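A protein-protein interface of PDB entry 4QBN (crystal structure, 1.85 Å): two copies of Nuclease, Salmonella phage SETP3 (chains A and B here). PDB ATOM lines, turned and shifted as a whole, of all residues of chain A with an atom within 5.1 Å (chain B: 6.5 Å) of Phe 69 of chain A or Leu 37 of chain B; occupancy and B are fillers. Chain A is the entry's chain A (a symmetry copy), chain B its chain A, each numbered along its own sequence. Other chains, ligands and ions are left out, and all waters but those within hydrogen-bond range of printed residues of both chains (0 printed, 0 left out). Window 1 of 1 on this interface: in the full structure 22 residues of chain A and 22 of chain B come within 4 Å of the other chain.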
ATOM      1  N   TYR A  27       0.019  37.781 -18.636  1.00  0.00           N
ATOM      2  CA  TYR A  27      -0.457  37.791 -20.005  1.00  0.00           C
ATOM      3  C   TYR A  27       0.235  38.905 -20.708  1.00  0.00           C
ATOM      4  O   TYR A  27       0.491  39.926 -20.082  1.00  0.00           O
ATOM      5  CB  TYR A  27      -1.937  38.089 -20.076  1.00  0.00           C
ATOM      6  CG  TYR A  27      -2.859  37.037 -19.529  1.00  0.00           C
ATOM      7  CD1 TYR A  27      -2.561  35.683 -19.611  1.00  0.00           C
ATOM      8  CD2 TYR A  27      -4.060  37.414 -18.940  1.00  0.00           C
ATOM      9  CE1 TYR A  27      -3.461  34.715 -19.110  1.00  0.00           C
ATOM     10  CE2 TYR A  27      -4.937  36.470 -18.452  1.00  0.00           C
ATOM     11  CZ  TYR A  27      -4.645  35.138 -18.539  1.00  0.00           C
ATOM     12  OH  TYR A  27      -5.546  34.186 -18.068  1.00  0.00           O
ATOM     13  N   PRO A  34      -3.910  33.991 -13.590  1.00  0.00           N
ATOM     14  CA  PRO A  34      -3.626  33.347 -12.289  1.00  0.00           C
ATOM     15  C   PRO A  34      -2.141  33.459 -11.900  1.00  0.00           C
ATOM     16  O   PRO A  34      -1.253  33.426 -12.758  1.00  0.00           O
ATOM     17  CB  PRO A  34      -3.980  31.865 -12.568  1.00  0.00           C
ATOM     18  CG  PRO A  34      -5.171  31.993 -13.562  1.00  0.00           C
ATOM     19  CD  PRO A  34      -4.784  33.184 -14.465  1.00  0.00           C
ATOM     20  N   PHE A  47      -4.322  26.086 -12.240  1.00  0.00           N
ATOM     21  CA  PHE A  47      -3.988  27.501 -12.216  1.00  0.00           C
ATOM     22  C   PHE A  47      -4.278  27.912 -10.798  1.00  0.00           C
ATOM     23  O   PHE A  47      -5.370  27.685 -10.306  1.00  0.00           O
ATOM     24  CB  PHE A  47      -4.923  28.242 -13.184  1.00  0.00           C
ATOM     25  CG  PHE A  47      -4.688  27.824 -14.617  1.00  0.00           C
ATOM     26  CD1 PHE A  47      -3.676  28.459 -15.350  1.00  0.00           C
ATOM     27  CD2 PHE A  47      -5.443  26.836 -15.199  1.00  0.00           C
ATOM     28  CE1 PHE A  47      -3.429  28.061 -16.660  1.00  0.00           C
ATOM     29  CE2 PHE A  47      -5.213  26.412 -16.520  1.00  0.00           C
ATOM     30  CZ  PHE A  47      -4.180  27.059 -17.258  1.00  0.00           C
ATOM     31  N   GLU A  65     -12.130  36.438 -14.742  1.00  0.00           N
ATOM     32  CA  GLU A  65     -11.191  35.561 -15.491  1.00  0.00           C
ATOM     33  C   GLU A  65     -11.237  34.102 -14.965  1.00  0.00           C
ATOM     34  O   GLU A  65     -11.317  33.122 -15.741  1.00  0.00           O
ATOM     35  CB  GLU A  65      -9.769  36.133 -15.393  1.00  0.00           C
ATOM     36  CG  GLU A  65      -8.740  35.342 -16.248  1.00  0.00           C
ATOM     37  CD  GLU A  65      -8.832  35.663 -17.764  1.00  0.00           C
ATOM     38  OE1 GLU A  65      -9.776  36.396 -18.190  1.00  0.00           O
ATOM     39  OE2 GLU A  65      -7.910  35.244 -18.540  1.00  0.00           O
ATOM     40  N   HIS A  66     -11.294  33.927 -13.647  1.00  0.00           N
ATOM     41  CA  HIS A  66     -11.395  32.536 -13.115  1.00  0.00           C
ATOM     42  C   HIS A  66     -12.650  31.883 -13.617  1.00  0.00           C
ATOM     43  O   HIS A  66     -12.683  30.690 -13.947  1.00  0.00           O
ATOM     44  CB  HIS A  66     -11.456  32.542 -11.572  1.00  0.00           C
ATOM     45  CG  HIS A  66     -10.242  33.107 -10.936  1.00  0.00           C
ATOM     46  ND1 HIS A  66     -10.176  33.381  -9.582  1.00  0.00           N
ATOM     47  CD2 HIS A  66      -9.051  33.475 -11.466  1.00  0.00           C
ATOM     48  CE1 HIS A  66      -8.987  33.897  -9.307  1.00  0.00           C
ATOM     49  NE2 HIS A  66      -8.279  33.956 -10.426  1.00  0.00           N
ATOM     50  N   GLU A  67     -13.728  32.650 -13.683  1.00  0.00           N
ATOM     51  CA  GLU A  67     -14.959  31.995 -14.143  1.00  0.00           C
ATOM     52  C   GLU A  67     -14.932  31.665 -15.642  1.00  0.00           C
ATOM     53  O   GLU A  67     -15.545  30.693 -16.030  1.00  0.00           O
ATOM     54  CB  GLU A  67     -16.222  32.735 -13.732  1.00  0.00           C
ATOM     55  CG  GLU A  67     -16.658  32.422 -12.236  1.00  0.00           C
ATOM     56  CD  GLU A  67     -17.085  30.945 -11.912  1.00  0.00           C
ATOM     57  OE1 GLU A  67     -18.283  30.631 -11.931  1.00  0.00           O
ATOM     58  OE2 GLU A  67     -16.258  30.114 -11.550  1.00  0.00           O
ATOM     59  N   ARG A  68     -14.289  32.485 -16.485  1.00  0.00           N
ATOM     60  CA  ARG A  68     -14.118  32.153 -17.912  1.00  0.00           C
ATOM     61  C   ARG A  68     -13.367  30.836 -18.065  1.00  0.00           C
ATOM     62  O   ARG A  68     -13.667  30.009 -18.978  1.00  0.00           O
ATOM     63  CB  ARG A  68     -13.313  33.249 -18.657  1.00  0.00           C
ATOM     64  CG  ARG A  68     -13.989  34.611 -18.709  1.00  0.00           C
ATOM     65  CD  ARG A  68     -13.158  35.565 -19.633  1.00  0.00           C
ATOM     66  NE  ARG A  68     -13.734  36.914 -19.673  1.00  0.00           N
ATOM     67  CZ  ARG A  68     -13.246  37.963 -18.997  1.00  0.00           C
ATOM     68  NH1 ARG A  68     -12.133  37.856 -18.238  1.00  0.00           N
ATOM     69  NH2 ARG A  68     -13.860  39.117 -19.093  1.00  0.00           N
ATOM     70  N   PHE A  69     -12.368  30.640 -17.211  1.00  0.00           N
ATOM     71  CA  PHE A  69     -11.596  29.399 -17.219  1.00  0.00           C
ATOM     72  C   PHE A  69     -12.484  28.233 -16.753  1.00  0.00           C
ATOM     73  O   PHE A  69     -12.500  27.152 -17.389  1.00  0.00           O
ATOM     74  CB  PHE A  69     -10.394  29.487 -16.258  1.00  0.00           C
ATOM     75  CG  PHE A  69      -9.129  30.092 -16.877  1.00  0.00           C
ATOM     76  CD1 PHE A  69      -9.179  31.271 -17.621  1.00  0.00           C
ATOM     77  CD2 PHE A  69      -7.885  29.500 -16.621  1.00  0.00           C
ATOM     78  CE1 PHE A  69      -7.978  31.823 -18.142  1.00  0.00           C
ATOM     79  CE2 PHE A  69      -6.728  30.045 -17.136  1.00  0.00           C
ATOM     80  CZ  PHE A  69      -6.777  31.218 -17.899  1.00  0.00           C
ATOM     81  N   ARG A  70     -13.163  28.410 -15.642  1.00  0.00           N
ATOM     82  CA  ARG A  70     -13.887  27.264 -15.053  1.00  0.00           C
ATOM     83  C   ARG A  70     -15.109  26.855 -15.892  1.00  0.00           C
ATOM     84  O   ARG A  70     -15.474  25.660 -15.917  1.00  0.00           O
ATOM     85  CB  ARG A  70     -14.299  27.552 -13.626  1.00  0.00           C
ATOM     86  CG  ARG A  70     -13.161  27.690 -12.621  1.00  0.00           C
ATOM     87  CD  ARG A  70     -13.792  27.562 -11.282  1.00  0.00           C
ATOM     88  NE  ARG A  70     -12.837  27.964 -10.238  1.00  0.00           N
ATOM     89  CZ  ARG A  70     -12.842  29.130  -9.623  1.00  0.00           C
ATOM     90  NH1 ARG A  70     -13.815  30.037  -9.872  1.00  0.00           N
ATOM     91  NH2 ARG A  70     -11.886  29.377  -8.725  1.00  0.00           N
ATOM     92  N   LYS A  71     -15.755  27.825 -16.558  1.00  0.00           N
ATOM     93  CA  LYS A  71     -16.888  27.526 -17.488  1.00  0.00           C
ATOM     94  C   LYS A  71     -16.496  26.513 -18.555  1.00  0.00           C
ATOM     95  O   LYS A  71     -17.316  25.678 -18.972  1.00  0.00           O
ATOM     96  CB  LYS A  71     -17.345  28.798 -18.210  1.00  0.00           C
ATOM     97  CG  LYS A  71     -18.059  29.781 -17.336  1.00  0.00           C
ATOM     98  CD  LYS A  71     -18.269  31.143 -18.054  1.00  0.00           C
ATOM     99  CE  LYS A  71     -19.235  32.038 -17.288  1.00  0.00           C
ATOM    100  NZ  LYS A  71     -19.541  33.281 -18.055  1.00  0.00           N
ATOM    101  N   ARG A  72     -15.236  26.560 -18.957  1.00  0.00           N
ATOM    102  CA  ARG A  72     -14.658  25.624 -19.926  1.00  0.00           C
ATOM    103  C   ARG A  72     -14.055  24.413 -19.313  1.00  0.00           C
ATOM    104  O   ARG A  72     -13.448  23.610 -20.005  1.00  0.00           O
ATOM    105  CB  ARG A  72     -13.591  26.361 -20.790  1.00  0.00           C
ATOM    106  CG  ARG A  72     -14.363  27.450 -21.685  1.00  0.00           C
ATOM    107  CD  ARG A  72     -13.441  28.516 -22.258  1.00  0.00           C
ATOM    108  NE  ARG A  72     -14.114  29.374 -23.191  1.00  0.00           N
ATOM    109  CZ  ARG A  72     -14.721  30.493 -22.851  1.00  0.00           C
ATOM    110  NH1 ARG A  72     -14.734  30.858 -21.596  1.00  0.00           N
ATOM    111  NH2 ARG A  72     -15.278  31.253 -23.767  1.00  0.00           N
ATOM    112  N   GLY A  73     -14.111  24.297 -17.990  1.00  0.00           N
ATOM    113  CA  GLY A  73     -13.679  23.054 -17.356  1.00  0.00           C
ATOM    114  C   GLY A  73     -12.291  23.078 -16.771  1.00  0.00           C
ATOM    115  O   GLY A  73     -11.746  22.048 -16.315  1.00  0.00           O
ATOM    116  N   ALA A  74     -11.656  24.246 -16.793  1.00  0.00           N
ATOM    117  CA  ALA A  74     -10.260  24.278 -16.296  1.00  0.00           C
ATOM    118  C   ALA A  74     -10.207  24.305 -14.759  1.00  0.00           C
ATOM    119  O   ALA A  74     -11.198  24.669 -14.121  1.00  0.00           O
ATOM    120  CB  ALA A  74      -9.508  25.536 -16.889  1.00  0.00           C
ATOM    121  N   VAL A  76      -9.072  25.947 -11.427  1.00  0.00           N
ATOM    122  CA  VAL A  76      -8.521  27.217 -10.965  1.00  0.00           C
ATOM    123  C   VAL A  76      -8.805  27.277  -9.482  1.00  0.00           C
ATOM    124  O   VAL A  76      -9.960  27.118  -9.064  1.00  0.00           O
ATOM    125  CB  VAL A  76      -9.251  28.390 -11.628  1.00  0.00           C
ATOM    126  CG1 VAL A  76      -8.704  29.669 -11.079  1.00  0.00           C
ATOM    127  CG2 VAL A  76      -9.111  28.299 -13.176  1.00  0.00           C
ATOM    128  N   LEU B  21     -11.007  29.689 -25.041  1.00  0.00           N
ATOM    129  CA  LEU B  21     -10.592  31.018 -24.547  1.00  0.00           C
ATOM    130  C   LEU B  21      -9.142  31.072 -24.954  1.00  0.00           C
ATOM    131  O   LEU B  21      -8.430  30.104 -24.712  1.00  0.00           O
ATOM    132  CB  LEU B  21     -10.672  31.014 -23.027  1.00  0.00           C
ATOM    133  CG  LEU B  21     -10.379  32.377 -22.379  1.00  0.00           C
ATOM    134  CD1 LEU B  21     -11.459  33.387 -22.762  1.00  0.00           C
ATOM    135  CD2 LEU B  21     -10.378  32.174 -20.881  1.00  0.00           C
ATOM    136  N   VAL B  22      -8.685  32.159 -25.558  1.00  0.00           N
ATOM    137  CA  VAL B  22      -7.268  32.206 -25.966  1.00  0.00           C
ATOM    138  C   VAL B  22      -6.572  33.356 -25.260  1.00  0.00           C
ATOM    139  O   VAL B  22      -7.126  34.458 -25.239  1.00  0.00           O
ATOM    140  CB  VAL B  22      -7.142  32.427 -27.458  1.00  0.00           C
ATOM    141  CG1 VAL B  22      -5.625  32.506 -27.881  1.00  0.00           C
ATOM    142  CG2 VAL B  22      -7.841  31.256 -28.177  1.00  0.00           C
ATOM    143  N   ARG B  23      -5.372  33.124 -24.699  1.00  0.00           N
ATOM    144  CA  ARG B  23      -4.635  34.228 -24.020  1.00  0.00           C
ATOM    145  C   ARG B  23      -3.183  34.221 -24.523  1.00  0.00           C
ATOM    146  O   ARG B  23      -2.637  33.137 -24.730  1.00  0.00           O
ATOM    147  CB  ARG B  23      -4.588  34.010 -22.502  1.00  0.00           C
ATOM    148  CG  ARG B  23      -6.014  34.111 -21.841  1.00  0.00           C
ATOM    149  CD  ARG B  23      -6.351  35.583 -21.803  1.00  0.00           C
ATOM    150  NE  ARG B  23      -7.682  35.854 -21.199  1.00  0.00           N
ATOM    151  CZ  ARG B  23      -8.806  36.042 -21.909  1.00  0.00           C
ATOM    152  NH1 ARG B  23      -8.805  35.928 -23.235  1.00  0.00           N
ATOM    153  NH2 ARG B  23      -9.945  36.341 -21.266  1.00  0.00           N
ATOM    154  N   LYS B  24      -2.604  35.404 -24.662  1.00  0.00           N
ATOM    155  CA  LYS B  24      -1.160  35.531 -24.975  1.00  0.00           C
ATOM    156  C   LYS B  24      -0.369  35.465 -23.669  1.00  0.00           C
ATOM    157  O   LYS B  24      -0.452  36.340 -22.817  1.00  0.00           O
ATOM    158  CB  LYS B  24      -0.883  36.803 -25.742  1.00  0.00           C
ATOM    159  CG  LYS B  24      -1.538  36.852 -27.131  1.00  0.00           C
ATOM    160  CD  LYS B  24      -1.240  38.215 -27.821  1.00  0.00           C
ATOM    161  CE  LYS B  24      -2.072  38.423 -29.097  1.00  0.00           C
ATOM    162  NZ  LYS B  24      -1.700  39.689 -29.868  1.00  0.00           N
ATOM    163  N   LEU B  25       0.460  34.438 -23.548  1.00  0.00           N
ATOM    164  CA  LEU B  25       1.101  34.086 -22.292  1.00  0.00           C
ATOM    165  C   LEU B  25       2.459  34.657 -22.179  1.00  0.00           C
ATOM    166  O   LEU B  25       3.167  34.816 -23.181  1.00  0.00           O
ATOM    167  CB  LEU B  25       1.188  32.550 -22.224  1.00  0.00           C
ATOM    168  CG  LEU B  25       0.947  31.890 -20.919  1.00  0.00           C
ATOM    169  CD1 LEU B  25      -0.396  32.363 -20.419  1.00  0.00           C
ATOM    170  CD2 LEU B  25       0.992  30.394 -21.214  1.00  0.00           C
ATOM    171  N   PRO B  34       5.017  29.370 -23.838  1.00  0.00           N
ATOM    172  CA  PRO B  34       4.323  29.208 -25.134  1.00  0.00           C
ATOM    173  C   PRO B  34       3.541  30.471 -25.533  1.00  0.00           C
ATOM    174  O   PRO B  34       2.997  31.180 -24.679  1.00  0.00           O
ATOM    175  CB  PRO B  34       3.333  28.054 -24.839  1.00  0.00           C
ATOM    176  CG  PRO B  34       4.141  27.175 -23.840  1.00  0.00           C
ATOM    177  CD  PRO B  34       4.883  28.197 -22.951  1.00  0.00           C
ATOM    178  N   ASP B  35       3.483  30.773 -26.832  1.00  0.00           N
ATOM    179  CA  ASP B  35       2.813  32.018 -27.267  1.00  0.00           C
ATOM    180  C   ASP B  35       1.357  32.081 -26.841  1.00  0.00           C
ATOM    181  O   ASP B  35       0.863  33.182 -26.452  1.00  0.00           O
ATOM    182  CB  ASP B  35       2.884  32.174 -28.793  1.00  0.00           C
ATOM    183  CG  ASP B  35       4.291  32.362 -29.273  1.00  0.00           C
ATOM    184  OD1 ASP B  35       4.983  33.181 -28.611  1.00  0.00           O
ATOM    185  OD2 ASP B  35       4.697  31.709 -30.280  1.00  0.00           O
ATOM    186  N   LEU B  36       0.631  30.957 -26.968  1.00  0.00           N
ATOM    187  CA  LEU B  36      -0.806  30.974 -26.669  1.00  0.00           C
ATOM    188  C   LEU B  36      -1.194  29.961 -25.621  1.00  0.00           C
ATOM    189  O   LEU B  36      -0.708  28.811 -25.640  1.00  0.00           O
ATOM    190  CB  LEU B  36      -1.618  30.647 -27.941  1.00  0.00           C
ATOM    191  CG  LEU B  36      -1.476  31.603 -29.110  1.00  0.00           C
ATOM    192  CD1 LEU B  36      -2.308  31.094 -30.290  1.00  0.00           C
ATOM    193  CD2 LEU B  36      -2.036  33.019 -28.716  1.00  0.00           C
ATOM    194  N   LEU B  37      -2.059  30.357 -24.685  1.00  0.00           N
ATOM    195  CA  LEU B  37      -2.750  29.375 -23.800  1.00  0.00           C
ATOM    196  C   LEU B  37      -4.153  29.269 -24.380  1.00  0.00           C
ATOM    197  O   LEU B  37      -4.772  30.311 -24.662  1.00  0.00           O
ATOM    198  CB  LEU B  37      -2.803  29.969 -22.378  1.00  0.00           C
ATOM    199  CG  LEU B  37      -3.775  29.238 -21.426  1.00  0.00           C
ATOM    200  CD1 LEU B  37      -3.322  27.786 -21.148  1.00  0.00           C
ATOM    201  CD2 LEU B  37      -3.867  30.079 -20.142  1.00  0.00           C
ATOM    202  N   VAL B  38      -4.629  28.041 -24.572  1.00  0.00           N
ATOM    203  CA  VAL B  38      -5.911  27.811 -25.217  1.00  0.00           C
ATOM    204  C   VAL B  38      -6.665  26.937 -24.242  1.00  0.00           C
ATOM    205  O   VAL B  38      -6.220  25.831 -23.909  1.00  0.00           O
ATOM    206  CB  VAL B  38      -5.765  27.066 -26.565  1.00  0.00           C
ATOM    207  CG1 VAL B  38      -7.107  26.910 -27.238  1.00  0.00           C
ATOM    208  CG2 VAL B  38      -4.835  27.892 -27.504  1.00  0.00           C
ATOM    209  N   ILE B  39      -7.813  27.421 -23.794  1.00  0.00           N
ATOM    210  CA  ILE B  39      -8.638  26.613 -22.856  1.00  0.00           C
ATOM    211  C   ILE B  39      -9.883  26.217 -23.633  1.00  0.00           C
ATOM    212  O   ILE B  39     -10.673  27.100 -23.958  1.00  0.00           O
ATOM    213  CB  ILE B  39      -9.108  27.434 -21.625  1.00  0.00           C
ATOM    214  CG1 ILE B  39      -7.976  28.231 -20.939  1.00  0.00           C
ATOM    215  CG2 ILE B  39      -9.880  26.490 -20.618  1.00  0.00           C
ATOM    216  CD1 ILE B  39      -7.086  27.440 -20.169  1.00  0.00           C
ATOM    217  N   ILE B  45      -6.596  21.608 -22.206  1.00  0.00           N
ATOM    218  CA  ILE B  45      -5.730  22.790 -22.128  1.00  0.00           C
ATOM    219  C   ILE B  45      -4.609  22.596 -23.158  1.00  0.00           C
ATOM    220  O   ILE B  45      -3.926  21.574 -23.086  1.00  0.00           O
ATOM    221  CB  ILE B  45      -5.052  22.854 -20.760  1.00  0.00           C
ATOM    222  CG1 ILE B  45      -6.060  22.786 -19.599  1.00  0.00           C
ATOM    223  CG2 ILE B  45      -4.203  24.136 -20.633  1.00  0.00           C
ATOM    224  CD1 ILE B  45      -7.001  23.950 -19.594  1.00  0.00           C
ATOM    225  N   TRP B  46      -4.414  23.543 -24.058  1.00  0.00           N
ATOM    226  CA  TRP B  46      -3.324  23.414 -25.070  1.00  0.00           C
ATOM    227  C   TRP B  46      -2.429  24.610 -24.910  1.00  0.00           C
ATOM    228  O   TRP B  46      -2.912  25.726 -24.668  1.00  0.00           O
ATOM    229  CB  TRP B  46      -3.871  23.441 -26.500  1.00  0.00           C
ATOM    230  CG  TRP B  46      -4.576  22.156 -26.971  1.00  0.00           C
ATOM    231  CD1 TRP B  46      -4.844  21.039 -26.236  1.00  0.00           C
ATOM    232  CD2 TRP B  46      -5.115  21.939 -28.263  1.00  0.00           C
ATOM    233  NE1 TRP B  46      -5.485  20.070 -27.032  1.00  0.00           N
ATOM    234  CE2 TRP B  46      -5.651  20.614 -28.288  1.00  0.00           C
ATOM    235  CE3 TRP B  46      -5.148  22.734 -29.440  1.00  0.00           C
ATOM    236  CZ2 TRP B  46      -6.219  20.039 -29.447  1.00  0.00           C
ATOM    237  CZ3 TRP B  46      -5.718  22.144 -30.614  1.00  0.00           C
ATOM    238  CH2 TRP B  46      -6.243  20.826 -30.591  1.00  0.00           C
ATOM    239  N   PHE B  47      -1.147  24.382 -25.105  1.00  0.00           N
ATOM    240  CA  PHE B  47      -0.197  25.482 -25.146  1.00  0.00           C
ATOM    241  C   PHE B  47       0.298  25.475 -26.566  1.00  0.00           C
ATOM    242  O   PHE B  47       0.753  24.453 -27.050  1.00  0.00           O
ATOM    243  CB  PHE B  47       0.957  25.170 -24.180  1.00  0.00           C
ATOM    244  CG  PHE B  47       0.487  25.131 -22.744  1.00  0.00           C
ATOM    245  CD1 PHE B  47       0.412  26.330 -22.023  1.00  0.00           C
ATOM    246  CD2 PHE B  47       0.134  23.945 -22.148  1.00  0.00           C
ATOM    247  CE1 PHE B  47      -0.049  26.310 -20.711  1.00  0.00           C
ATOM    248  CE2 PHE B  47      -0.337  23.897 -20.824  1.00  0.00           C
ATOM    249  CZ  PHE B  47      -0.415  25.120 -20.098  1.00  0.00           C
ATOM    250  N   VAL B  48       0.213  26.603 -27.227  1.00  0.00           N
ATOM    251  CA  VAL B  48       0.533  26.622 -28.665  1.00  0.00           C
ATOM    252  C   VAL B  48       1.604  27.664 -28.981  1.00  0.00           C
ATOM    253  O   VAL B  48       1.459  28.838 -28.646  1.00  0.00           O
ATOM    254  CB  VAL B  48      -0.744  26.916 -29.496  1.00  0.00           C
ATOM    255  CG1 VAL B  48      -0.362  27.009 -31.003  1.00  0.00           C
ATOM    256  CG2 VAL B  48      -1.727  25.773 -29.272  1.00  0.00           C
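Among the printed residues, pairs that only touch across the chains: Tyr 27 of chain A with Lys 24 of chain B, Arg 72 of chain A with Ile 39 of chain B, Phe 69 of chain A with Leu 21 of chain B, Arg 72 of chain A with Leu 21 of chain B, Tyr 27 of chain A with Arg 23 of chain B, Arg 68 of chain A with Arg 23 of chain B, Arg 68 of chain A with Leu 21 of chain B, Phe 69 of chain A with Leu 37 of chain B and Ala 74 of chain A with Ile 39 of chain B.
The side-chain carboxylate (OE2) of Glu 65 of chain A is in salt-bridge range of the guanidinium group (NE) of Arg 23 of chain B (2.7 Å).
O of Arg 23 of chain B lies within hydrogen-bond range of N of Leu 37 of chain B (2.8 Å).
OE1 of Glu 65 of chain A lies within salt-bridge range of NH1 of Arg 68 of chain A, at 2.8 Å.
The backbone carbonyl oxygen of Phe 69 of chain A is in hydrogen-bond range of the backbone NH of Ala 74 of chain A.
O of Ile 39 of chain B is in hydrogen-bond range of N of Leu 21 of chain B.
OH of Tyr 27 of chain A is in hydrogen-bond range of OE2 of Glu 65 of chain A (2.6 Å).
The guanidinium group (NH1) of Arg 72 of chain A lies within hydrogen-bond range of the backbone carbonyl oxygen (O) of Arg 68 of chain A.
Of the printed residues of chain B, Tyr 27 of chain A touches Arg 23 and Lys 24.
Printed residues of chain B within 4 Å of Phe 69 of chain A: Leu 21 and Leu 37.
Of the printed residues of chain B, Ala 74 of chain A touches Ile 39 (3.9 Å).
Val 76 of chain A touches none of the printed residues of chain B.
Of the printed residues of chain A, Leu 21 of chain B touches Arg 68, Phe 69 and Arg 72.
Leu 25 of chain B touches none of the printed residues of chain A.
Printed residues of chain A within 4 Å of Leu 37 of chain B: Phe 69 (3.8 Å).
The nearest printed residue of chain B that does not touch Phe 69 of chain A is Ile 39 of chain B (4.01 Å).
The nearest residue of chain A that does not touch Leu 37 of chain B is Phe 47 of chain A (4.05 Å).
Of the 14 printed residues of chain A, 6 touch a printed residue of chain B.
Along chain A the printed residues that touch a printed residue of chain B span positions 27 to 74.
Among the printed residues, 10 pairs touch across the chains.
Among the printed residues, Asp or Glu carboxylates within 4 Å of a Lys or Arg side-chain nitrogen of the other chain: Glu 65 of chain A with Arg 23 of chain B.
2 positions are printed for both chains.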
